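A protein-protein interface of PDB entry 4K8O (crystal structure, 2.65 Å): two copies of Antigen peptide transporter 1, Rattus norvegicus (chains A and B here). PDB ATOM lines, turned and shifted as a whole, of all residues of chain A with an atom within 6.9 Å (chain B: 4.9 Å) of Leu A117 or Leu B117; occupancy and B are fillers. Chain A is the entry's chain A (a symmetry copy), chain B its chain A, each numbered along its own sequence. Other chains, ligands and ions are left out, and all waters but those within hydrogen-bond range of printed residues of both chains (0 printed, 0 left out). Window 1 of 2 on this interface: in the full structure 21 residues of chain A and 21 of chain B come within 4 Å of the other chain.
Of the 16 printed residues of chain A, 5 touch a printed residue of chain B. Hydrophobic or aromatic side chains of chain B within 4 Å of the printed part of chain A: Tyr B115. Among the printed residues, no Asp or Glu carboxylate lies within 4 Å of a Lys or Arg side-chain nitrogen of the other chain.
Among the printed residues, merely in contact across the chains: Tyr A115 with Thr B118, Thr A118 with Tyr B115, Leu A117 with Thr B118, Thr A118 with Leu B117, His A89 with Tyr B115, His A89 with Arg B173, Leu A117 with Leu B117, Thr A120 with Arg B119 and His A89 with Gly B116.
The guanidinium group (NH1) of Arg B173 sits at hydrogen-bond distance from the backbone carbonyl oxygen (O) of Gly B116 (2.9 Å). The guanidinium group (NH2) of Arg B119 sits at hydrogen-bond distance from the backbone carbonyl oxygen (O) of Ile B172 (3.3 Å). The guanidinium group of Arg B173 lies within hydrogen-bond range of the side-chain hydroxyl of Thr B118. The guanidinium group (NH1) of Arg A173 sits at hydrogen-bond distance from the side-chain hydroxyl (OG1) of Thr A118 (3.2 Å).
Of chain B, only Leu B117 (3.7 Å) and Thr B118 (3.3 Å) come within 4 Å of Leu A117. Of chain A, only Leu A117 (3.7 Å) and Thr A118 (3.3 Å) come within 4 Å of Leu B117. Gly B116 touches one residue of chain A. Of the printed residues of chain A, Arg B119 touches Thr A120. Printed residues of chain B within 4 Å of Thr A120: Arg B119 (3.8 Å). Printed residues of chain B within 4 Å of Thr A118: Tyr B115 (3.2 Å) and Leu B117 (3.3 Å). The nearest residue of chain B that does not touch Leu A117 is Arg B119 (4.3 Å). The nearest residue of chain A that does not touch Leu B117 is Arg A119 (4.3 Å). The nearest printed residue of chain B that does not touch Tyr A115 is Arg B119 (7.5 Å).
Tyr A115 touches Thr B118, and with the chains exchanged Thr A118 touches Tyr B115. Leu A117 touches its own counterpart, Leu B117. Leu A117 touches Thr B118, and with the chains exchanged Thr A118 touches Leu B117. Of the 9 pairs that touch across the chains among the printed residues, 5 have their exchanged pair printed and touching as well.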
ATOM      1  N   HIS A  89      15.830  18.104   3.455  1.00  0.00           N
ATOM      2  CA  HIS A  89      15.770  17.435   4.751  1.00  0.00           C
ATOM      3  C   HIS A  89      16.907  17.863   5.672  1.00  0.00           C
ATOM      4  O   HIS A  89      16.792  17.770   6.893  1.00  0.00           O
ATOM      5  CB  HIS A  89      15.751  15.916   4.579  1.00  0.00           C
ATOM      6  CG  HIS A  89      14.421  15.376   4.153  1.00  0.00           C
ATOM      7  ND1 HIS A  89      13.463  14.966   5.054  1.00  0.00           N
ATOM      8  CD2 HIS A  89      13.887  15.191   2.923  1.00  0.00           C
ATOM      9  CE1 HIS A  89      12.396  14.544   4.397  1.00  0.00           C
ATOM     10  NE2 HIS A  89      12.628  14.670   3.103  1.00  0.00           N
ATOM     11  N   ILE A 113       6.259  15.971  20.344  1.00  0.00           N
ATOM     12  CA  ILE A 113       7.536  16.619  20.623  1.00  0.00           C
ATOM     13  C   ILE A 113       8.638  16.098  19.702  1.00  0.00           C
ATOM     14  O   ILE A 113       9.415  16.879  19.151  1.00  0.00           O
ATOM     15  CB  ILE A 113       7.955  16.436  22.098  1.00  0.00           C
ATOM     16  CG1 ILE A 113       6.967  17.150  23.022  1.00  0.00           C
ATOM     17  CG2 ILE A 113       9.362  16.965  22.330  1.00  0.00           C
ATOM     18  CD1 ILE A 113       7.280  16.988  24.495  1.00  0.00           C
ATOM     19  N   ALA A 114       8.697  14.779  19.537  1.00  0.00           N
ATOM     20  CA  ALA A 114       9.665  14.155  18.639  1.00  0.00           C
ATOM     21  C   ALA A 114       9.490  14.682  17.220  1.00  0.00           C
ATOM     22  O   ALA A 114      10.455  15.106  16.584  1.00  0.00           O
ATOM     23  CB  ALA A 114       9.519  12.642  18.667  1.00  0.00           C
ATOM     24  N   TYR A 115       8.250  14.647  16.740  1.00  0.00           N
ATOM     25  CA  TYR A 115       7.876  15.246  15.459  1.00  0.00           C
ATOM     26  C   TYR A 115       8.668  14.688  14.278  1.00  0.00           C
ATOM     27  O   TYR A 115       8.546  13.511  13.941  1.00  0.00           O
ATOM     28  CB  TYR A 115       8.015  16.770  15.526  1.00  0.00           C
ATOM     29  CG  TYR A 115       7.229  17.510  14.470  1.00  0.00           C
ATOM     30  CD1 TYR A 115       5.894  17.208  14.234  1.00  0.00           C
ATOM     31  CD2 TYR A 115       7.815  18.522  13.721  1.00  0.00           C
ATOM     32  CE1 TYR A 115       5.170  17.884  13.274  1.00  0.00           C
ATOM     33  CE2 TYR A 115       7.097  19.206  12.761  1.00  0.00           C
ATOM     34  CZ  TYR A 115       5.775  18.882  12.540  1.00  0.00           C
ATOM     35  OH  TYR A 115       5.056  19.561  11.583  1.00  0.00           O
ATOM     36  N   GLY A 116       9.475  15.539  13.654  1.00  0.00           N
ATOM     37  CA  GLY A 116      10.241  15.146  12.485  1.00  0.00           C
ATOM     38  C   GLY A 116      11.699  14.867  12.794  1.00  0.00           C
ATOM     39  O   GLY A 116      12.562  15.001  11.925  1.00  0.00           O
ATOM     40  N   LEU A 117      11.972  14.474  14.034  1.00  0.00           N
ATOM     41  CA  LEU A 117      13.330  14.166  14.470  1.00  0.00           C
ATOM     42  C   LEU A 117      13.915  12.996  13.679  1.00  0.00           C
ATOM     43  O   LEU A 117      13.221  12.021  13.394  1.00  0.00           O
ATOM     44  CB  LEU A 117      13.345  13.852  15.968  1.00  0.00           C
ATOM     45  CG  LEU A 117      14.706  13.816  16.661  1.00  0.00           C
ATOM     46  CD1 LEU A 117      15.420  15.145  16.502  1.00  0.00           C
ATOM     47  CD2 LEU A 117      14.544  13.474  18.132  1.00  0.00           C
ATOM     48  N   THR A 118      15.196  13.101  13.332  1.00  0.00           N
ATOM     49  CA  THR A 118      15.866  12.091  12.517  1.00  0.00           C
ATOM     50  C   THR A 118      16.474  10.983  13.376  1.00  0.00           C
ATOM     51  O   THR A 118      17.496  10.396  13.020  1.00  0.00           O
ATOM     52  CB  THR A 118      16.976  12.720  11.651  1.00  0.00           C
ATOM     53  OG1 THR A 118      16.631  14.073  11.335  1.00  0.00           O
ATOM     54  CG2 THR A 118      17.163  11.938  10.362  1.00  0.00           C
ATOM     55  N   ARG A 119      15.842  10.705  14.511  1.00  0.00           N
ATOM     56  CA  ARG A 119      16.307   9.670  15.425  1.00  0.00           C
ATOM     57  C   ARG A 119      15.213   9.348  16.433  1.00  0.00           C
ATOM     58  O   ARG A 119      14.148   9.964  16.422  1.00  0.00           O
ATOM     59  CB  ARG A 119      17.565  10.131  16.164  1.00  0.00           C
ATOM     60  CG  ARG A 119      17.318  11.285  17.119  1.00  0.00           C
ATOM     61  CD  ARG A 119      18.583  11.712  17.844  1.00  0.00           C
ATOM     62  NE  ARG A 119      18.311  12.779  18.804  1.00  0.00           N
ATOM     63  CZ  ARG A 119      18.335  14.074  18.508  1.00  0.00           C
ATOM     64  NH1 ARG A 119      18.620  14.470  17.275  1.00  0.00           N
ATOM     65  NH2 ARG A 119      18.071  14.975  19.444  1.00  0.00           N
ATOM     66  N   THR A 120      15.479   8.382  17.305  1.00  0.00           N
ATOM     67  CA  THR A 120      14.552   8.056  18.380  1.00  0.00           C
ATOM     68  C   THR A 120      15.065   8.635  19.692  1.00  0.00           C
ATOM     69  O   THR A 120      16.117   8.230  20.185  1.00  0.00           O
ATOM     70  CB  THR A 120      14.359   6.536  18.524  1.00  0.00           C
ATOM     71  OG1 THR A 120      13.855   5.996  17.296  1.00  0.00           O
ATOM     72  CG2 THR A 120      13.377   6.229  19.646  1.00  0.00           C
ATOM     73  N   PRO A 121      14.320   9.595  20.263  1.00  0.00           N
ATOM     74  CA  PRO A 121      14.752  10.288  21.479  1.00  0.00           C
ATOM     75  C   PRO A 121      14.357   9.548  22.752  1.00  0.00           C
ATOM     76  O   PRO A 121      13.273   8.971  22.825  1.00  0.00           O
ATOM     77  CB  PRO A 121      14.011  11.625  21.392  1.00  0.00           C
ATOM     78  CG  PRO A 121      12.805  11.360  20.513  1.00  0.00           C
ATOM     79  CD  PRO A 121      12.976  10.020  19.839  1.00  0.00           C
ATOM     80  N   THR A 122      15.242   9.568  23.744  1.00  0.00           N
ATOM     81  CA  THR A 122      14.968   8.937  25.028  1.00  0.00           C
ATOM     82  C   THR A 122      13.978   9.778  25.825  1.00  0.00           C
ATOM     83  O   THR A 122      13.726  10.936  25.491  1.00  0.00           O
ATOM     84  CB  THR A 122      16.254   8.758  25.853  1.00  0.00           C
ATOM     85  OG1 THR A 122      16.753  10.040  26.253  1.00  0.00           O
ATOM     86  CG2 THR A 122      17.315   8.035  25.036  1.00  0.00           C
ATOM     87  N   GLU A 125      15.427  12.784  27.306  1.00  0.00           N
ATOM     88  CA  GLU A 125      15.598  13.823  26.302  1.00  0.00           C
ATOM     89  C   GLU A 125      14.296  14.589  26.085  1.00  0.00           C
ATOM     90  O   GLU A 125      14.298  15.814  25.967  1.00  0.00           O
ATOM     91  CB  GLU A 125      16.070  13.192  24.991  1.00  0.00           C
ATOM     92  CG  GLU A 125      16.802  14.131  24.053  1.00  0.00           C
ATOM     93  CD  GLU A 125      17.636  13.377  23.037  1.00  0.00           C
ATOM     94  OE1 GLU A 125      18.116  12.272  23.369  1.00  0.00           O
ATOM     95  OE2 GLU A 125      17.807  13.883  21.908  1.00  0.00           O
ATOM     96  N   ARG A 169       8.996  21.015  20.778  1.00  0.00           N
ATOM     97  CA  ARG A 169       9.115  20.316  19.505  1.00  0.00           C
ATOM     98  C   ARG A 169      10.335  20.788  18.719  1.00  0.00           C
ATOM     99  O   ARG A 169      11.024  19.990  18.083  1.00  0.00           O
ATOM    100  CB  ARG A 169       7.844  20.524  18.679  1.00  0.00           C
ATOM    101  CG  ARG A 169       7.913  19.978  17.266  1.00  0.00           C
ATOM    102  CD  ARG A 169       6.664  20.339  16.480  1.00  0.00           C
ATOM    103  NE  ARG A 169       5.467  19.701  17.020  1.00  0.00           N
ATOM    104  CZ  ARG A 169       4.247  19.850  16.511  1.00  0.00           C
ATOM    105  NH1 ARG A 169       4.059  20.621  15.449  1.00  0.00           N
ATOM    106  NH2 ARG A 169       3.215  19.231  17.067  1.00  0.00           N
ATOM    107  N   ILE A 172      14.024  20.099  20.829  1.00  0.00           N
ATOM    108  CA  ILE A 172      14.594  18.758  20.731  1.00  0.00           C
ATOM    109  C   ILE A 172      15.299  18.539  19.392  1.00  0.00           C
ATOM    110  O   ILE A 172      16.126  17.636  19.251  1.00  0.00           O
ATOM    111  CB  ILE A 172      13.513  17.672  20.948  1.00  0.00           C
ATOM    112  CG1 ILE A 172      14.156  16.331  21.313  1.00  0.00           C
ATOM    113  CG2 ILE A 172      12.621  17.542  19.723  1.00  0.00           C
ATOM    114  CD1 ILE A 172      13.155  15.236  21.616  1.00  0.00           C
ATOM    115  N   ARG A 173      14.972  19.377  18.412  1.00  0.00           N
ATOM    116  CA  ARG A 173      15.612  19.321  17.105  1.00  0.00           C
ATOM    117  C   ARG A 173      17.035  19.860  17.180  1.00  0.00           C
ATOM    118  O   ARG A 173      17.875  19.536  16.338  1.00  0.00           O
ATOM    119  CB  ARG A 173      14.810  20.129  16.083  1.00  0.00           C
ATOM    120  CG  ARG A 173      13.641  19.378  15.470  1.00  0.00           C
ATOM    121  CD  ARG A 173      14.133  18.241  14.591  1.00  0.00           C
ATOM    122  NE  ARG A 173      13.703  18.381  13.202  1.00  0.00           N
ATOM    123  CZ  ARG A 173      14.098  17.583  12.217  1.00  0.00           C
ATOM    124  NH1 ARG A 173      14.937  16.587  12.468  1.00  0.00           N
ATOM    125  NH2 ARG A 173      13.654  17.780  10.981  1.00  0.00           N
ATOM    126  N   LYS A 174      17.293  20.670  18.205  1.00  0.00           N
ATOM    127  CA  LYS A 174      18.562  21.382  18.357  1.00  0.00           C
ATOM    128  C   LYS A 174      18.979  22.083  17.066  1.00  0.00           C
ATOM    129  O   LYS A 174      20.035  21.784  16.506  1.00  0.00           O
ATOM    130  CB  LYS A 174      19.663  20.435  18.839  1.00  0.00           C
ATOM    131  CG  LYS A 174      19.612  20.147  20.329  1.00  0.00           C
ATOM    132  CD  LYS A 174      20.475  18.954  20.700  1.00  0.00           C
ATOM    133  CE  LYS A 174      19.876  17.662  20.172  1.00  0.00           C
ATOM    134  NZ  LYS A 174      20.627  16.464  20.641  1.00  0.00           N
ATOM    135  N   ALA B 114      19.288   6.270   5.280  1.00  0.00           N
ATOM    136  CA  ALA B 114      18.414   6.679   6.377  1.00  0.00           C
ATOM    137  C   ALA B 114      17.770   8.025   6.070  1.00  0.00           C
ATOM    138  O   ALA B 114      16.553   8.178   6.174  1.00  0.00           O
ATOM    139  CB  ALA B 114      19.192   6.747   7.681  1.00  0.00           C
ATOM    140  N   TYR B 115      18.603   8.991   5.692  1.00  0.00           N
ATOM    141  CA  TYR B 115      18.144  10.296   5.217  1.00  0.00           C
ATOM    142  C   TYR B 115      17.273  11.035   6.232  1.00  0.00           C
ATOM    143  O   TYR B 115      17.743  11.415   7.303  1.00  0.00           O
ATOM    144  CB  TYR B 115      17.405  10.146   3.885  1.00  0.00           C
ATOM    145  CG  TYR B 115      17.309  11.422   3.083  1.00  0.00           C
ATOM    146  CD1 TYR B 115      18.429  12.213   2.867  1.00  0.00           C
ATOM    147  CD2 TYR B 115      16.103  11.827   2.525  1.00  0.00           C
ATOM    148  CE1 TYR B 115      18.349  13.377   2.132  1.00  0.00           C
ATOM    149  CE2 TYR B 115      16.014  12.988   1.785  1.00  0.00           C
ATOM    150  CZ  TYR B 115      17.139  13.760   1.591  1.00  0.00           C
ATOM    151  OH  TYR B 115      17.054  14.920   0.855  1.00  0.00           O
ATOM    152  N   GLY B 116      16.006  11.235   5.887  1.00  0.00           N
ATOM    153  CA  GLY B 116      15.090  11.971   6.740  1.00  0.00           C
ATOM    154  C   GLY B 116      14.147  11.073   7.516  1.00  0.00           C
ATOM    155  O   GLY B 116      13.046  11.485   7.882  1.00  0.00           O
ATOM    156  N   LEU B 117      14.584   9.844   7.772  1.00  0.00           N
ATOM    157  CA  LEU B 117      13.784   8.874   8.513  1.00  0.00           C
ATOM    158  C   LEU B 117      13.497   9.361   9.933  1.00  0.00           C
ATOM    159  O   LEU B 117      14.367   9.935  10.588  1.00  0.00           O
ATOM    160  CB  LEU B 117      14.499   7.521   8.552  1.00  0.00           C
ATOM    161  CG  LEU B 117      13.682   6.312   9.006  1.00  0.00           C
ATOM    162  CD1 LEU B 117      12.469   6.123   8.114  1.00  0.00           C
ATOM    163  CD2 LEU B 117      14.541   5.060   9.005  1.00  0.00           C
ATOM    164  N   THR B 118      12.276   9.124  10.403  1.00  0.00           N
ATOM    165  CA  THR B 118      11.842   9.593  11.717  1.00  0.00           C
ATOM    166  C   THR B 118      12.161   8.578  12.813  1.00  0.00           C
ATOM    167  O   THR B 118      11.442   8.474  13.807  1.00  0.00           O
ATOM    168  CB  THR B 118      10.327   9.886  11.732  1.00  0.00           C
ATOM    169  OG1 THR B 118       9.903  10.293  10.426  1.00  0.00           O
ATOM    170  CG2 THR B 118      10.001  10.986  12.727  1.00  0.00           C
ATOM    171  N   ARG B 119      13.243   7.830  12.625  1.00  0.00           N
ATOM    172  CA  ARG B 119      13.669   6.826  13.591  1.00  0.00           C
ATOM    173  C   ARG B 119      15.094   6.390  13.280  1.00  0.00           C
ATOM    174  O   ARG B 119      15.692   6.844  12.305  1.00  0.00           O
ATOM    175  CB  ARG B 119      12.742   5.610  13.547  1.00  0.00           C
ATOM    176  CG  ARG B 119      12.825   4.829  12.247  1.00  0.00           C
ATOM    177  CD  ARG B 119      11.901   3.624  12.240  1.00  0.00           C
ATOM    178  NE  ARG B 119      12.043   2.852  11.008  1.00  0.00           N
ATOM    179  CZ  ARG B 119      11.352   3.084   9.897  1.00  0.00           C
ATOM    180  NH1 ARG B 119      10.463   4.067   9.859  1.00  0.00           N
ATOM    181  NH2 ARG B 119      11.550   2.333   8.823  1.00  0.00           N
ATOM    182  N   PRO B 121      17.228   3.309  12.064  1.00  0.00           N
ATOM    183  CA  PRO B 121      17.060   2.012  11.404  1.00  0.00           C
ATOM    184  C   PRO B 121      18.201   1.045  11.704  1.00  0.00           C
ATOM    185  O   PRO B 121      19.358   1.455  11.784  1.00  0.00           O
ATOM    186  CB  PRO B 121      17.055   2.380   9.919  1.00  0.00           C
ATOM    187  CG  PRO B 121      17.801   3.696   9.829  1.00  0.00           C
ATOM    188  CD  PRO B 121      17.969   4.259  11.220  1.00  0.00           C
ATOM    189  N   ILE B 172      13.190   2.714   2.363  1.00  0.00           N
ATOM    190  CA  ILE B 172      13.263   2.585   3.817  1.00  0.00           C
ATOM    191  C   ILE B 172      12.255   3.497   4.517  1.00  0.00           C
ATOM    192  O   ILE B 172      11.914   3.288   5.683  1.00  0.00           O
ATOM    193  CB  ILE B 172      14.692   2.874   4.334  1.00  0.00           C
ATOM    194  CG1 ILE B 172      14.889   2.296   5.738  1.00  0.00           C
ATOM    195  CG2 ILE B 172      14.989   4.365   4.304  1.00  0.00           C
ATOM    196  CD1 ILE B 172      16.291   2.473   6.281  1.00  0.00           C
ATOM    197  N   ARG B 173      11.774   4.505   3.795  1.00  0.00           N
ATOM    198  CA  ARG B 173      10.762   5.412   4.317  1.00  0.00           C
ATOM    199  C   ARG B 173       9.404   4.724   4.380  1.00  0.00           C
ATOM    200  O   ARG B 173       8.528   5.132   5.146  1.00  0.00           O
ATOM    201  CB  ARG B 173      10.664   6.664   3.442  1.00  0.00           C
ATOM    202  CG  ARG B 173      11.693   7.733   3.760  1.00  0.00           C
ATOM    203  CD  ARG B 173      11.433   8.339   5.130  1.00  0.00           C
ATOM    204  NE  ARG B 173      11.173   9.774   5.065  1.00  0.00           N
ATOM    205  CZ  ARG B 173      10.806  10.512   6.107  1.00  0.00           C
ATOM    206  NH1 ARG B 173      10.650   9.945   7.297  1.00  0.00           N
ATOM    207  NH2 ARG B 173      10.594  11.814   5.961  1.00  0.00           N
